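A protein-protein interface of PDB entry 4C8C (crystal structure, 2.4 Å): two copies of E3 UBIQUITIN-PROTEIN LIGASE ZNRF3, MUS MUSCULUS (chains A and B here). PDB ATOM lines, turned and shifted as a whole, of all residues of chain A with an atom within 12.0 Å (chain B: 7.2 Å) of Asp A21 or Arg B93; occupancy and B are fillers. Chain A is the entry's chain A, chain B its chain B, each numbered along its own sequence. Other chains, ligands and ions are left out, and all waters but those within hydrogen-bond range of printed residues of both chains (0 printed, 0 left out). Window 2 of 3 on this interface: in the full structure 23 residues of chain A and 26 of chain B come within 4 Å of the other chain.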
ATOM      1  N   VAL A  12      39.541 -26.123 -20.887  1.00  0.00           N
ATOM      2  CA  VAL A  12      38.499 -25.171 -21.259  1.00  0.00           C
ATOM      3  C   VAL A  12      38.014 -24.438 -19.999  1.00  0.00           C
ATOM      4  O   VAL A  12      37.608 -25.060 -19.021  1.00  0.00           O
ATOM      5  CB  VAL A  12      37.303 -25.907 -21.865  1.00  0.00           C
ATOM      6  CG1 VAL A  12      36.349 -24.953 -22.540  1.00  0.00           C
ATOM      7  CG2 VAL A  12      37.767 -26.945 -22.884  1.00  0.00           C
ATOM      8  N   LEU A  13      38.104 -23.118 -20.015  1.00  0.00           N
ATOM      9  CA  LEU A  13      37.501 -22.284 -18.968  1.00  0.00           C
ATOM     10  C   LEU A  13      36.187 -21.648 -19.499  1.00  0.00           C
ATOM     11  O   LEU A  13      36.088 -21.348 -20.659  1.00  0.00           O
ATOM     12  CB  LEU A  13      38.521 -21.238 -18.490  1.00  0.00           C
ATOM     13  CG  LEU A  13      39.820 -21.785 -17.855  1.00  0.00           C
ATOM     14  CD1 LEU A  13      40.835 -20.688 -17.549  1.00  0.00           C
ATOM     15  CD2 LEU A  13      39.545 -22.570 -16.598  1.00  0.00           C
ATOM     16  N   PHE A  14      35.157 -21.512 -18.679  1.00  0.00           N
ATOM     17  CA  PHE A  14      33.873 -21.101 -19.203  1.00  0.00           C
ATOM     18  C   PHE A  14      33.143 -20.169 -18.238  1.00  0.00           C
ATOM     19  O   PHE A  14      33.132 -20.416 -17.021  1.00  0.00           O
ATOM     20  CB  PHE A  14      33.013 -22.333 -19.533  1.00  0.00           C
ATOM     21  CG  PHE A  14      33.033 -23.398 -18.468  1.00  0.00           C
ATOM     22  CD1 PHE A  14      32.160 -23.348 -17.393  1.00  0.00           C
ATOM     23  CD2 PHE A  14      33.931 -24.474 -18.541  1.00  0.00           C
ATOM     24  CE1 PHE A  14      32.178 -24.331 -16.407  1.00  0.00           C
ATOM     25  CE2 PHE A  14      33.948 -25.456 -17.557  1.00  0.00           C
ATOM     26  CZ  PHE A  14      33.077 -25.373 -16.485  1.00  0.00           C
ATOM     27  N   GLU A  15      32.547 -19.098 -18.781  1.00  0.00           N
ATOM     28  CA  GLU A  15      31.603 -18.227 -18.030  1.00  0.00           C
ATOM     29  C   GLU A  15      30.286 -18.213 -18.769  1.00  0.00           C
ATOM     30  O   GLU A  15      30.271 -17.995 -19.977  1.00  0.00           O
ATOM     31  CB  GLU A  15      32.075 -16.757 -17.936  1.00  0.00           C
ATOM     32  CG  GLU A  15      33.557 -16.510 -17.667  1.00  0.00           C
ATOM     33  CD  GLU A  15      34.006 -15.120 -18.106  1.00  0.00           C
ATOM     34  OE1 GLU A  15      33.653 -14.128 -17.419  1.00  0.00           O
ATOM     35  OE2 GLU A  15      34.714 -15.022 -19.140  1.00  0.00           O
ATOM     36  N   SER A  16      29.181 -18.418 -18.057  1.00  0.00           N
ATOM     37  CA  SER A  16      27.855 -18.130 -18.639  1.00  0.00           C
ATOM     38  C   SER A  16      27.623 -16.648 -18.584  1.00  0.00           C
ATOM     39  O   SER A  16      28.255 -15.952 -17.793  1.00  0.00           O
ATOM     40  CB  SER A  16      26.722 -18.831 -17.892  1.00  0.00           C
ATOM     41  OG  SER A  16      26.988 -18.851 -16.501  1.00  0.00           O
ATOM     42  N   SER A  17      26.754 -16.172 -19.467  1.00  0.00           N
ATOM     43  CA  SER A  17      26.144 -14.862 -19.349  1.00  0.00           C
ATOM     44  C   SER A  17      24.844 -15.079 -18.570  1.00  0.00           C
ATOM     45  O   SER A  17      24.451 -16.226 -18.322  1.00  0.00           O
ATOM     46  CB  SER A  17      25.873 -14.276 -20.735  1.00  0.00           C
ATOM     47  OG  SER A  17      24.794 -14.943 -21.386  1.00  0.00           O
ATOM     48  N   PRO A  18      24.176 -13.984 -18.159  1.00  0.00           N
ATOM     49  CA  PRO A  18      22.864 -14.119 -17.503  1.00  0.00           C
ATOM     50  C   PRO A  18      21.854 -14.815 -18.412  1.00  0.00           C
ATOM     51  O   PRO A  18      21.138 -15.702 -17.966  1.00  0.00           O
ATOM     52  CB  PRO A  18      22.456 -12.670 -17.236  1.00  0.00           C
ATOM     53  CG  PRO A  18      23.745 -11.917 -17.173  1.00  0.00           C
ATOM     54  CD  PRO A  18      24.648 -12.584 -18.170  1.00  0.00           C
ATOM     55  N   SER A  19      21.839 -14.425 -19.687  1.00  0.00           N
ATOM     56  CA  SER A  19      21.039 -15.088 -20.733  1.00  0.00           C
ATOM     57  C   SER A  19      21.228 -16.617 -20.845  1.00  0.00           C
ATOM     58  O   SER A  19      20.423 -17.284 -21.489  1.00  0.00           O
ATOM     59  CB  SER A  19      21.316 -14.442 -22.107  1.00  0.00           C
ATOM     60  OG  SER A  19      22.565 -14.860 -22.645  1.00  0.00           O
ATOM     61  N   GLY A  20      22.289 -17.169 -20.253  1.00  0.00           N
ATOM     62  CA  GLY A  20      22.541 -18.616 -20.308  1.00  0.00           C
ATOM     63  C   GLY A  20      23.559 -19.055 -21.366  1.00  0.00           C
ATOM     64  O   GLY A  20      23.965 -20.211 -21.402  1.00  0.00           O
ATOM     65  N   ASP A  21      23.981 -18.133 -22.226  1.00  0.00           N
ATOM     66  CA  ASP A  21      24.911 -18.449 -23.295  1.00  0.00           C
ATOM     67  C   ASP A  21      26.309 -18.525 -22.699  1.00  0.00           C
ATOM     68  O   ASP A  21      26.623 -17.762 -21.815  1.00  0.00           O
ATOM     69  CB  ASP A  21      24.802 -17.386 -24.407  1.00  0.00           C
ATOM     70  CG  ASP A  21      23.391 -17.333 -25.040  1.00  0.00           C
ATOM     71  OD1 ASP A  21      22.570 -18.260 -24.766  1.00  0.00           O
ATOM     72  OD2 ASP A  21      23.097 -16.370 -25.812  1.00  0.00           O
ATOM     73  N   TYR A  22      27.138 -19.464 -23.162  1.00  0.00           N
ATOM     74  CA  TYR A  22      28.482 -19.670 -22.575  1.00  0.00           C
ATOM     75  C   TYR A  22      29.608 -19.134 -23.382  1.00  0.00           C
ATOM     76  O   TYR A  22      29.576 -19.111 -24.611  1.00  0.00           O
ATOM     77  CB  TYR A  22      28.815 -21.140 -22.377  1.00  0.00           C
ATOM     78  CG  TYR A  22      28.254 -21.715 -21.150  1.00  0.00           C
ATOM     79  CD1 TYR A  22      28.876 -21.536 -19.943  1.00  0.00           C
ATOM     80  CD2 TYR A  22      27.076 -22.435 -21.185  1.00  0.00           C
ATOM     81  CE1 TYR A  22      28.338 -22.088 -18.781  1.00  0.00           C
ATOM     82  CE2 TYR A  22      26.550 -23.000 -20.048  1.00  0.00           C
ATOM     83  CZ  TYR A  22      27.185 -22.807 -18.846  1.00  0.00           C
ATOM     84  OH  TYR A  22      26.664 -23.355 -17.715  1.00  0.00           O
ATOM     85  N   THR A  23      30.654 -18.795 -22.655  1.00  0.00           N
ATOM     86  CA  THR A  23      31.823 -18.219 -23.238  1.00  0.00           C
ATOM     87  C   THR A  23      33.006 -19.001 -22.665  1.00  0.00           C
ATOM     88  O   THR A  23      33.136 -19.126 -21.434  1.00  0.00           O
ATOM     89  CB  THR A  23      31.856 -16.686 -22.961  1.00  0.00           C
ATOM     90  OG1 THR A  23      32.382 -16.008 -24.108  1.00  0.00           O
ATOM     91  CG2 THR A  23      32.667 -16.309 -21.704  1.00  0.00           C
ATOM     92  N   THR A  24      33.831 -19.541 -23.570  1.00  0.00           N
ATOM     93  CA  THR A  24      34.933 -20.442 -23.224  1.00  0.00           C
ATOM     94  C   THR A  24      36.322 -19.945 -23.664  1.00  0.00           C
ATOM     95  O   THR A  24      36.439 -19.177 -24.610  1.00  0.00           O
ATOM     96  CB  THR A  24      34.727 -21.832 -23.860  1.00  0.00           C
ATOM     97  OG1 THR A  24      34.658 -21.713 -25.287  1.00  0.00           O
ATOM     98  CG2 THR A  24      33.458 -22.503 -23.325  1.00  0.00           C
ATOM     99  N   HIS A  25      37.359 -20.405 -22.961  1.00  0.00           N
ATOM    100  CA  HIS A  25      38.763 -20.128 -23.281  1.00  0.00           C
ATOM    101  C   HIS A  25      39.547 -21.445 -23.230  1.00  0.00           C
ATOM    102  O   HIS A  25      39.780 -22.032 -22.147  1.00  0.00           O
ATOM    103  CB  HIS A  25      39.352 -19.094 -22.307  1.00  0.00           C
ATOM    104  CG  HIS A  25      40.854 -18.974 -22.352  1.00  0.00           C
ATOM    105  ND1 HIS A  25      41.517 -18.160 -23.247  1.00  0.00           N
ATOM    106  CD2 HIS A  25      41.815 -19.543 -21.584  1.00  0.00           C
ATOM    107  CE1 HIS A  25      42.819 -18.246 -23.040  1.00  0.00           C
ATOM    108  NE2 HIS A  25      43.025 -19.069 -22.027  1.00  0.00           N
ATOM    109  N   GLY B  53      12.153 -25.587 -27.649  1.00  0.00           N
ATOM    110  CA  GLY B  53      13.017 -25.685 -26.461  1.00  0.00           C
ATOM    111  C   GLY B  53      14.452 -25.310 -26.786  1.00  0.00           C
ATOM    112  O   GLY B  53      15.252 -25.002 -25.899  1.00  0.00           O
ATOM    113  N   LEU B  54      14.777 -25.352 -28.071  1.00  0.00           N
ATOM    114  CA  LEU B  54      15.963 -24.703 -28.586  1.00  0.00           C
ATOM    115  C   LEU B  54      15.516 -23.570 -29.520  1.00  0.00           C
ATOM    116  O   LEU B  54      15.751 -23.636 -30.716  1.00  0.00           O
ATOM    117  CB  LEU B  54      16.868 -25.735 -29.299  1.00  0.00           C
ATOM    118  CG  LEU B  54      17.471 -26.816 -28.390  1.00  0.00           C
ATOM    119  CD1 LEU B  54      18.155 -27.872 -29.236  1.00  0.00           C
ATOM    120  CD2 LEU B  54      18.441 -26.246 -27.355  1.00  0.00           C
ATOM    121  N   CYS B  55      14.838 -22.554 -28.978  1.00  0.00           N
ATOM    122  CA  CYS B  55      14.567 -21.318 -29.734  1.00  0.00           C
ATOM    123  C   CYS B  55      14.759 -20.104 -28.825  1.00  0.00           C
ATOM    124  O   CYS B  55      15.848 -19.892 -28.295  1.00  0.00           O
ATOM    125  CB  CYS B  55      13.158 -21.290 -30.371  1.00  0.00           C
ATOM    126  SG  CYS B  55      12.361 -22.879 -30.762  1.00  0.00           S
ATOM    127  N   LEU B  63      20.776 -22.265 -17.729  1.00  0.00           N
ATOM    128  CA  LEU B  63      20.068 -23.321 -17.028  1.00  0.00           C
ATOM    129  C   LEU B  63      20.903 -24.614 -16.998  1.00  0.00           C
ATOM    130  O   LEU B  63      20.517 -25.576 -16.326  1.00  0.00           O
ATOM    131  CB  LEU B  63      18.687 -23.544 -17.692  1.00  0.00           C
ATOM    132  CG  LEU B  63      17.504 -24.289 -17.007  1.00  0.00           C
ATOM    133  CD1 LEU B  63      17.009 -23.686 -15.689  1.00  0.00           C
ATOM    134  CD2 LEU B  63      16.332 -24.377 -17.978  1.00  0.00           C
ATOM    135  N   TRP B  68      27.546 -30.501 -21.404  1.00  0.00           N
ATOM    136  CA  TRP B  68      26.555 -31.533 -21.541  1.00  0.00           C
ATOM    137  C   TRP B  68      26.556 -32.035 -23.020  1.00  0.00           C
ATOM    138  O   TRP B  68      26.998 -31.340 -23.942  1.00  0.00           O
ATOM    139  CB  TRP B  68      25.171 -31.044 -21.143  1.00  0.00           C
ATOM    140  CG  TRP B  68      24.719 -29.734 -21.688  1.00  0.00           C
ATOM    141  CD1 TRP B  68      25.045 -28.478 -21.215  1.00  0.00           C
ATOM    142  CD2 TRP B  68      23.787 -29.520 -22.767  1.00  0.00           C
ATOM    143  NE1 TRP B  68      24.416 -27.493 -21.991  1.00  0.00           N
ATOM    144  CE2 TRP B  68      23.641 -28.109 -22.935  1.00  0.00           C
ATOM    145  CE3 TRP B  68      23.144 -30.378 -23.667  1.00  0.00           C
ATOM    146  CZ2 TRP B  68      22.832 -27.554 -23.900  1.00  0.00           C
ATOM    147  CZ3 TRP B  68      22.333 -29.827 -24.630  1.00  0.00           C
ATOM    148  CH2 TRP B  68      22.161 -28.413 -24.720  1.00  0.00           C
ATOM    149  N   LEU B  85      13.941 -22.402 -35.711  1.00  0.00           N
ATOM    150  CA  LEU B  85      15.281 -22.496 -36.342  1.00  0.00           C
ATOM    151  C   LEU B  85      15.411 -23.738 -37.210  1.00  0.00           C
ATOM    152  O   LEU B  85      14.776 -24.759 -36.939  1.00  0.00           O
ATOM    153  CB  LEU B  85      16.371 -22.567 -35.268  1.00  0.00           C
ATOM    154  CG  LEU B  85      16.397 -21.493 -34.164  1.00  0.00           C
ATOM    155  CD1 LEU B  85      17.310 -21.860 -32.997  1.00  0.00           C
ATOM    156  CD2 LEU B  85      16.815 -20.158 -34.770  1.00  0.00           C
ATOM    157  N   LEU B  88      19.779 -27.320 -38.002  1.00  0.00           N
ATOM    158  CA  LEU B  88      21.181 -26.887 -37.912  1.00  0.00           C
ATOM    159  C   LEU B  88      21.316 -25.714 -36.919  1.00  0.00           C
ATOM    160  O   LEU B  88      22.314 -25.578 -36.205  1.00  0.00           O
ATOM    161  CB  LEU B  88      21.692 -26.447 -39.293  1.00  0.00           C
ATOM    162  CG  LEU B  88      23.041 -25.705 -39.315  1.00  0.00           C
ATOM    163  CD1 LEU B  88      24.146 -26.690 -38.944  1.00  0.00           C
ATOM    164  CD2 LEU B  88      23.335 -24.997 -40.640  1.00  0.00           C
ATOM    165  N   GLY B  89      20.310 -24.854 -36.915  1.00  0.00           N
ATOM    166  CA  GLY B  89      20.246 -23.760 -35.983  1.00  0.00           C
ATOM    167  C   GLY B  89      20.115 -24.267 -34.577  1.00  0.00           C
ATOM    168  O   GLY B  89      20.729 -23.720 -33.662  1.00  0.00           O
ATOM    169  N   LYS B  90      19.304 -25.305 -34.398  1.00  0.00           N
ATOM    170  CA  LYS B  90      19.013 -25.821 -33.058  1.00  0.00           C
ATOM    171  C   LYS B  90      20.302 -26.282 -32.427  1.00  0.00           C
ATOM    172  O   LYS B  90      20.534 -26.055 -31.246  1.00  0.00           O
ATOM    173  CB  LYS B  90      18.038 -26.974 -33.126  1.00  0.00           C
ATOM    174  CG  LYS B  90      16.623 -26.512 -33.414  1.00  0.00           C
ATOM    175  CD  LYS B  90      15.667 -27.677 -33.612  1.00  0.00           C
ATOM    176  CE  LYS B  90      14.317 -27.221 -34.170  1.00  0.00           C
ATOM    177  NZ  LYS B  90      13.788 -26.019 -33.459  1.00  0.00           N
ATOM    178  N   ALA B  91      21.168 -26.893 -33.236  1.00  0.00           N
ATOM    179  CA  ALA B  91      22.420 -27.391 -32.730  1.00  0.00           C
ATOM    180  C   ALA B  91      23.396 -26.308 -32.276  1.00  0.00           C
ATOM    181  O   ALA B  91      24.093 -26.489 -31.284  1.00  0.00           O
ATOM    182  CB  ALA B  91      23.067 -28.289 -33.775  1.00  0.00           C
ATOM    183  N   LYS B  92      23.494 -25.206 -33.005  1.00  0.00           N
ATOM    184  CA  LYS B  92      24.370 -24.120 -32.597  1.00  0.00           C
ATOM    185  C   LYS B  92      23.821 -23.501 -31.313  1.00  0.00           C
ATOM    186  O   LYS B  92      24.518 -23.107 -30.401  1.00  0.00           O
ATOM    187  CB  LYS B  92      24.405 -23.040 -33.656  1.00  0.00           C
ATOM    188  CG  LYS B  92      24.642 -23.550 -35.073  1.00  0.00           C
ATOM    189  CD  LYS B  92      25.079 -22.444 -36.025  1.00  0.00           C
ATOM    190  CE  LYS B  92      25.147 -22.950 -37.468  1.00  0.00           C
ATOM    191  NZ  LYS B  92      25.864 -22.014 -38.381  1.00  0.00           N
ATOM    192  N   ARG B  93      22.528 -23.382 -31.271  1.00  0.00           N
ATOM    193  CA  ARG B  93      21.918 -22.826 -30.122  1.00  0.00           C
ATOM    194  C   ARG B  93      22.311 -23.634 -28.869  1.00  0.00           C
ATOM    195  O   ARG B  93      22.607 -23.060 -27.798  1.00  0.00           O
ATOM    196  CB  ARG B  93      20.413 -22.811 -30.345  1.00  0.00           C
ATOM    197  CG  ARG B  93      19.683 -21.929 -29.373  1.00  0.00           C
ATOM    198  CD  ARG B  93      20.388 -20.608 -29.202  1.00  0.00           C
ATOM    199  NE  ARG B  93      19.721 -19.915 -28.134  1.00  0.00           N
ATOM    200  CZ  ARG B  93      20.305 -19.103 -27.279  1.00  0.00           C
ATOM    201  NH1 ARG B  93      21.588 -18.796 -27.380  1.00  0.00           N
ATOM    202  NH2 ARG B  93      19.561 -18.572 -26.322  1.00  0.00           N
ATOM    203  N   ALA B  94      22.355 -24.962 -29.038  1.00  0.00           N
ATOM    204  CA  ALA B  94      22.636 -25.902 -27.967  1.00  0.00           C
ATOM    205  C   ALA B  94      24.063 -25.765 -27.527  1.00  0.00           C
ATOM    206  O   ALA B  94      24.370 -25.645 -26.306  1.00  0.00           O
ATOM    207  CB  ALA B  94      22.373 -27.307 -28.433  1.00  0.00           C
ATOM    208  N   VAL B  95      24.954 -25.772 -28.517  1.00  0.00           N
ATOM    209  CA  VAL B  95      26.365 -25.452 -28.272  1.00  0.00           C
ATOM    210  C   VAL B  95      26.547 -24.049 -27.609  1.00  0.00           C
ATOM    211  O   VAL B  95      27.394 -23.846 -26.762  1.00  0.00           O
ATOM    212  CB  VAL B  95      27.179 -25.544 -29.590  1.00  0.00           C
ATOM    213  CG1 VAL B  95      28.532 -24.881 -29.440  1.00  0.00           C
ATOM    214  CG2 VAL B  95      27.315 -27.020 -30.062  1.00  0.00           C
ATOM    215  N   GLN B  96      25.812 -23.068 -28.057  1.00  0.00           N
ATOM    216  CA  GLN B  96      25.855 -21.738 -27.412  1.00  0.00           C
ATOM    217  C   GLN B  96      25.563 -21.870 -25.928  1.00  0.00           C
ATOM    218  O   GLN B  96      26.149 -21.224 -25.136  1.00  0.00           O
ATOM    219  CB  GLN B  96      24.825 -20.810 -28.033  1.00  0.00           C
ATOM    220  CG  GLN B  96      25.414 -19.895 -29.061  1.00  0.00           C
ATOM    221  CD  GLN B  96      24.354 -19.123 -29.828  1.00  0.00           C
ATOM    222  OE1 GLN B  96      23.150 -19.315 -29.617  1.00  0.00           O
ATOM    223  NE2 GLN B  96      24.798 -18.264 -30.756  1.00  0.00           N
ATOM    224  N   ARG B  97      24.687 -22.783 -25.597  1.00  0.00           N
ATOM    225  CA  ARG B  97      24.300 -23.032 -24.254  1.00  0.00           C
ATOM    226  C   ARG B  97      25.083 -24.141 -23.573  1.00  0.00           C
ATOM    227  O   ARG B  97      24.514 -24.896 -22.778  1.00  0.00           O
ATOM    228  CB  ARG B  97      22.797 -23.337 -24.288  1.00  0.00           C
ATOM    229  CG  ARG B  97      22.065 -22.044 -24.608  1.00  0.00           C
ATOM    230  CD  ARG B  97      20.585 -22.251 -24.815  1.00  0.00           C
ATOM    231  NE  ARG B  97      19.924 -23.182 -23.878  1.00  0.00           N
ATOM    232  CZ  ARG B  97      18.762 -23.809 -24.132  1.00  0.00           C
ATOM    233  NH1 ARG B  97      18.101 -23.614 -25.278  1.00  0.00           N
ATOM    234  NH2 ARG B  97      18.246 -24.642 -23.231  1.00  0.00           N
ATOM    235  N   GLY B  98      26.370 -24.273 -23.925  1.00  0.00           N
ATOM    236  CA  GLY B  98      27.289 -25.228 -23.248  1.00  0.00           C
ATOM    237  C   GLY B  98      27.300 -26.693 -23.706  1.00  0.00           C
ATOM    238  O   GLY B  98      27.948 -27.559 -23.117  1.00  0.00           O
ATOM    239  N   ALA B  99      26.563 -27.011 -24.731  1.00  0.00           N
ATOM    240  CA  ALA B  99      26.491 -28.398 -25.110  1.00  0.00           C
ATOM    241  C   ALA B  99      27.876 -28.788 -25.631  1.00  0.00           C
ATOM    242  O   ALA B  99      28.448 -28.090 -26.470  1.00  0.00           O
ATOM    243  CB  ALA B  99      25.439 -28.567 -26.147  1.00  0.00           C
ATOM    244  N   VAL B 102      25.983 -32.389 -29.837  1.00  0.00           N
ATOM    245  CA  VAL B 102      24.521 -32.602 -29.938  1.00  0.00           C
ATOM    246  C   VAL B 102      24.268 -33.886 -30.721  1.00  0.00           C
ATOM    247  O   VAL B 102      24.958 -34.139 -31.694  1.00  0.00           O
ATOM    248  CB  VAL B 102      23.803 -31.455 -30.679  1.00  0.00           C
ATOM    249  CG1 VAL B 102      22.298 -31.638 -30.643  1.00  0.00           C
ATOM    250  CG2 VAL B 102      24.169 -30.089 -30.118  1.00  0.00           C
ATOM    251  N   LEU B 124      30.344 -26.139 -37.234  1.00  0.00           N
ATOM    252  CA  LEU B 124      30.421 -25.995 -35.786  1.00  0.00           C
ATOM    253  C   LEU B 124      31.683 -26.621 -35.207  1.00  0.00           C
ATOM    254  O   LEU B 124      32.153 -27.683 -35.643  1.00  0.00           O
ATOM    255  CB  LEU B 124      29.205 -26.666 -35.153  1.00  0.00           C
ATOM    256  CG  LEU B 124      28.047 -25.752 -34.769  1.00  0.00           C
ATOM    257  CD1 LEU B 124      26.888 -26.605 -34.273  1.00  0.00           C
ATOM    258  CD2 LEU B 124      28.550 -24.772 -33.704  1.00  0.00           C
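No position is printed for both chains.
Of chain B, only Arg B93 (2.8 Å), Gln B96 (3.6 Å) and Arg B97 (3.8 Å) come within 4 Å of Asp A21. No residue of chain B comes within 4 Å of Gly A20. No residue of chain A comes within 4 Å of Leu B54. No residue of chain A comes within 4 Å of Gly B89. Ala B91 touches none of the printed residues of chain A. No residue of chain A comes within 4 Å of Ala B94. No residue of chain A comes within 4 Å of Val B95. Of chain A, only Asp A21 and Tyr A22 come within 4 Å of Gln B96. Of the printed residues of chain B, Tyr A22 touches Gln B96 (2.8 Å), Arg B97 (3.5 Å) and Gly B98 (3.4 Å). Printed residues of chain A within 4 Å of Gly B98: Tyr A22. Phe A14 touches none of the printed residues of chain B. The nearest residue of chain B that does not touch Asp A21 is Gly B98 (5.9 Å). The nearest printed residue of chain B that does not touch Tyr A22 is Trp B68 (5.3 Å).
OG of Ser A17 sits at hydrogen-bond distance from O of Asp A21, 3.4 Å away. The guanidinium group of Arg B97 sits at hydrogen-bond distance from the backbone carbonyl oxygen of Gly B53 (3.2 Å). The backbone carbonyl oxygen of Arg B97 sits at hydrogen-bond distance from the indole nitrogen of Trp B68, at 2.7 Å. O of Gly B98 sits at hydrogen-bond distance from N of Trp B68 (3.4 Å). NH1 of Arg B93 sits at hydrogen-bond distance from OE1 of Gln B96.
The side-chain carboxylate (OD1) of Asp A21 is in salt-bridge range of the guanidinium group (NH1) of Arg B93. O of Gln B96 is in hydrogen-bond range of N of Tyr A22, at 2.8 Å.
Hydrophobic or aromatic side chains of chain A that line the printed part of chain B: Tyr A22. Along chain A the printed residues that touch a printed residue of chain B span positions 21 to 22. Of the 20 printed residues of chain B, 4 touch a printed residue of chain A.
Asp A21 touches Gln B96 (CA to O, 3.6 Å). Arg B97 touches Asp A21. CD2 of Tyr A22 touches C of Arg B97, 3.5 Å away. Tyr A22 touches Gly B98 (CD2 to N, 3.4 Å).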
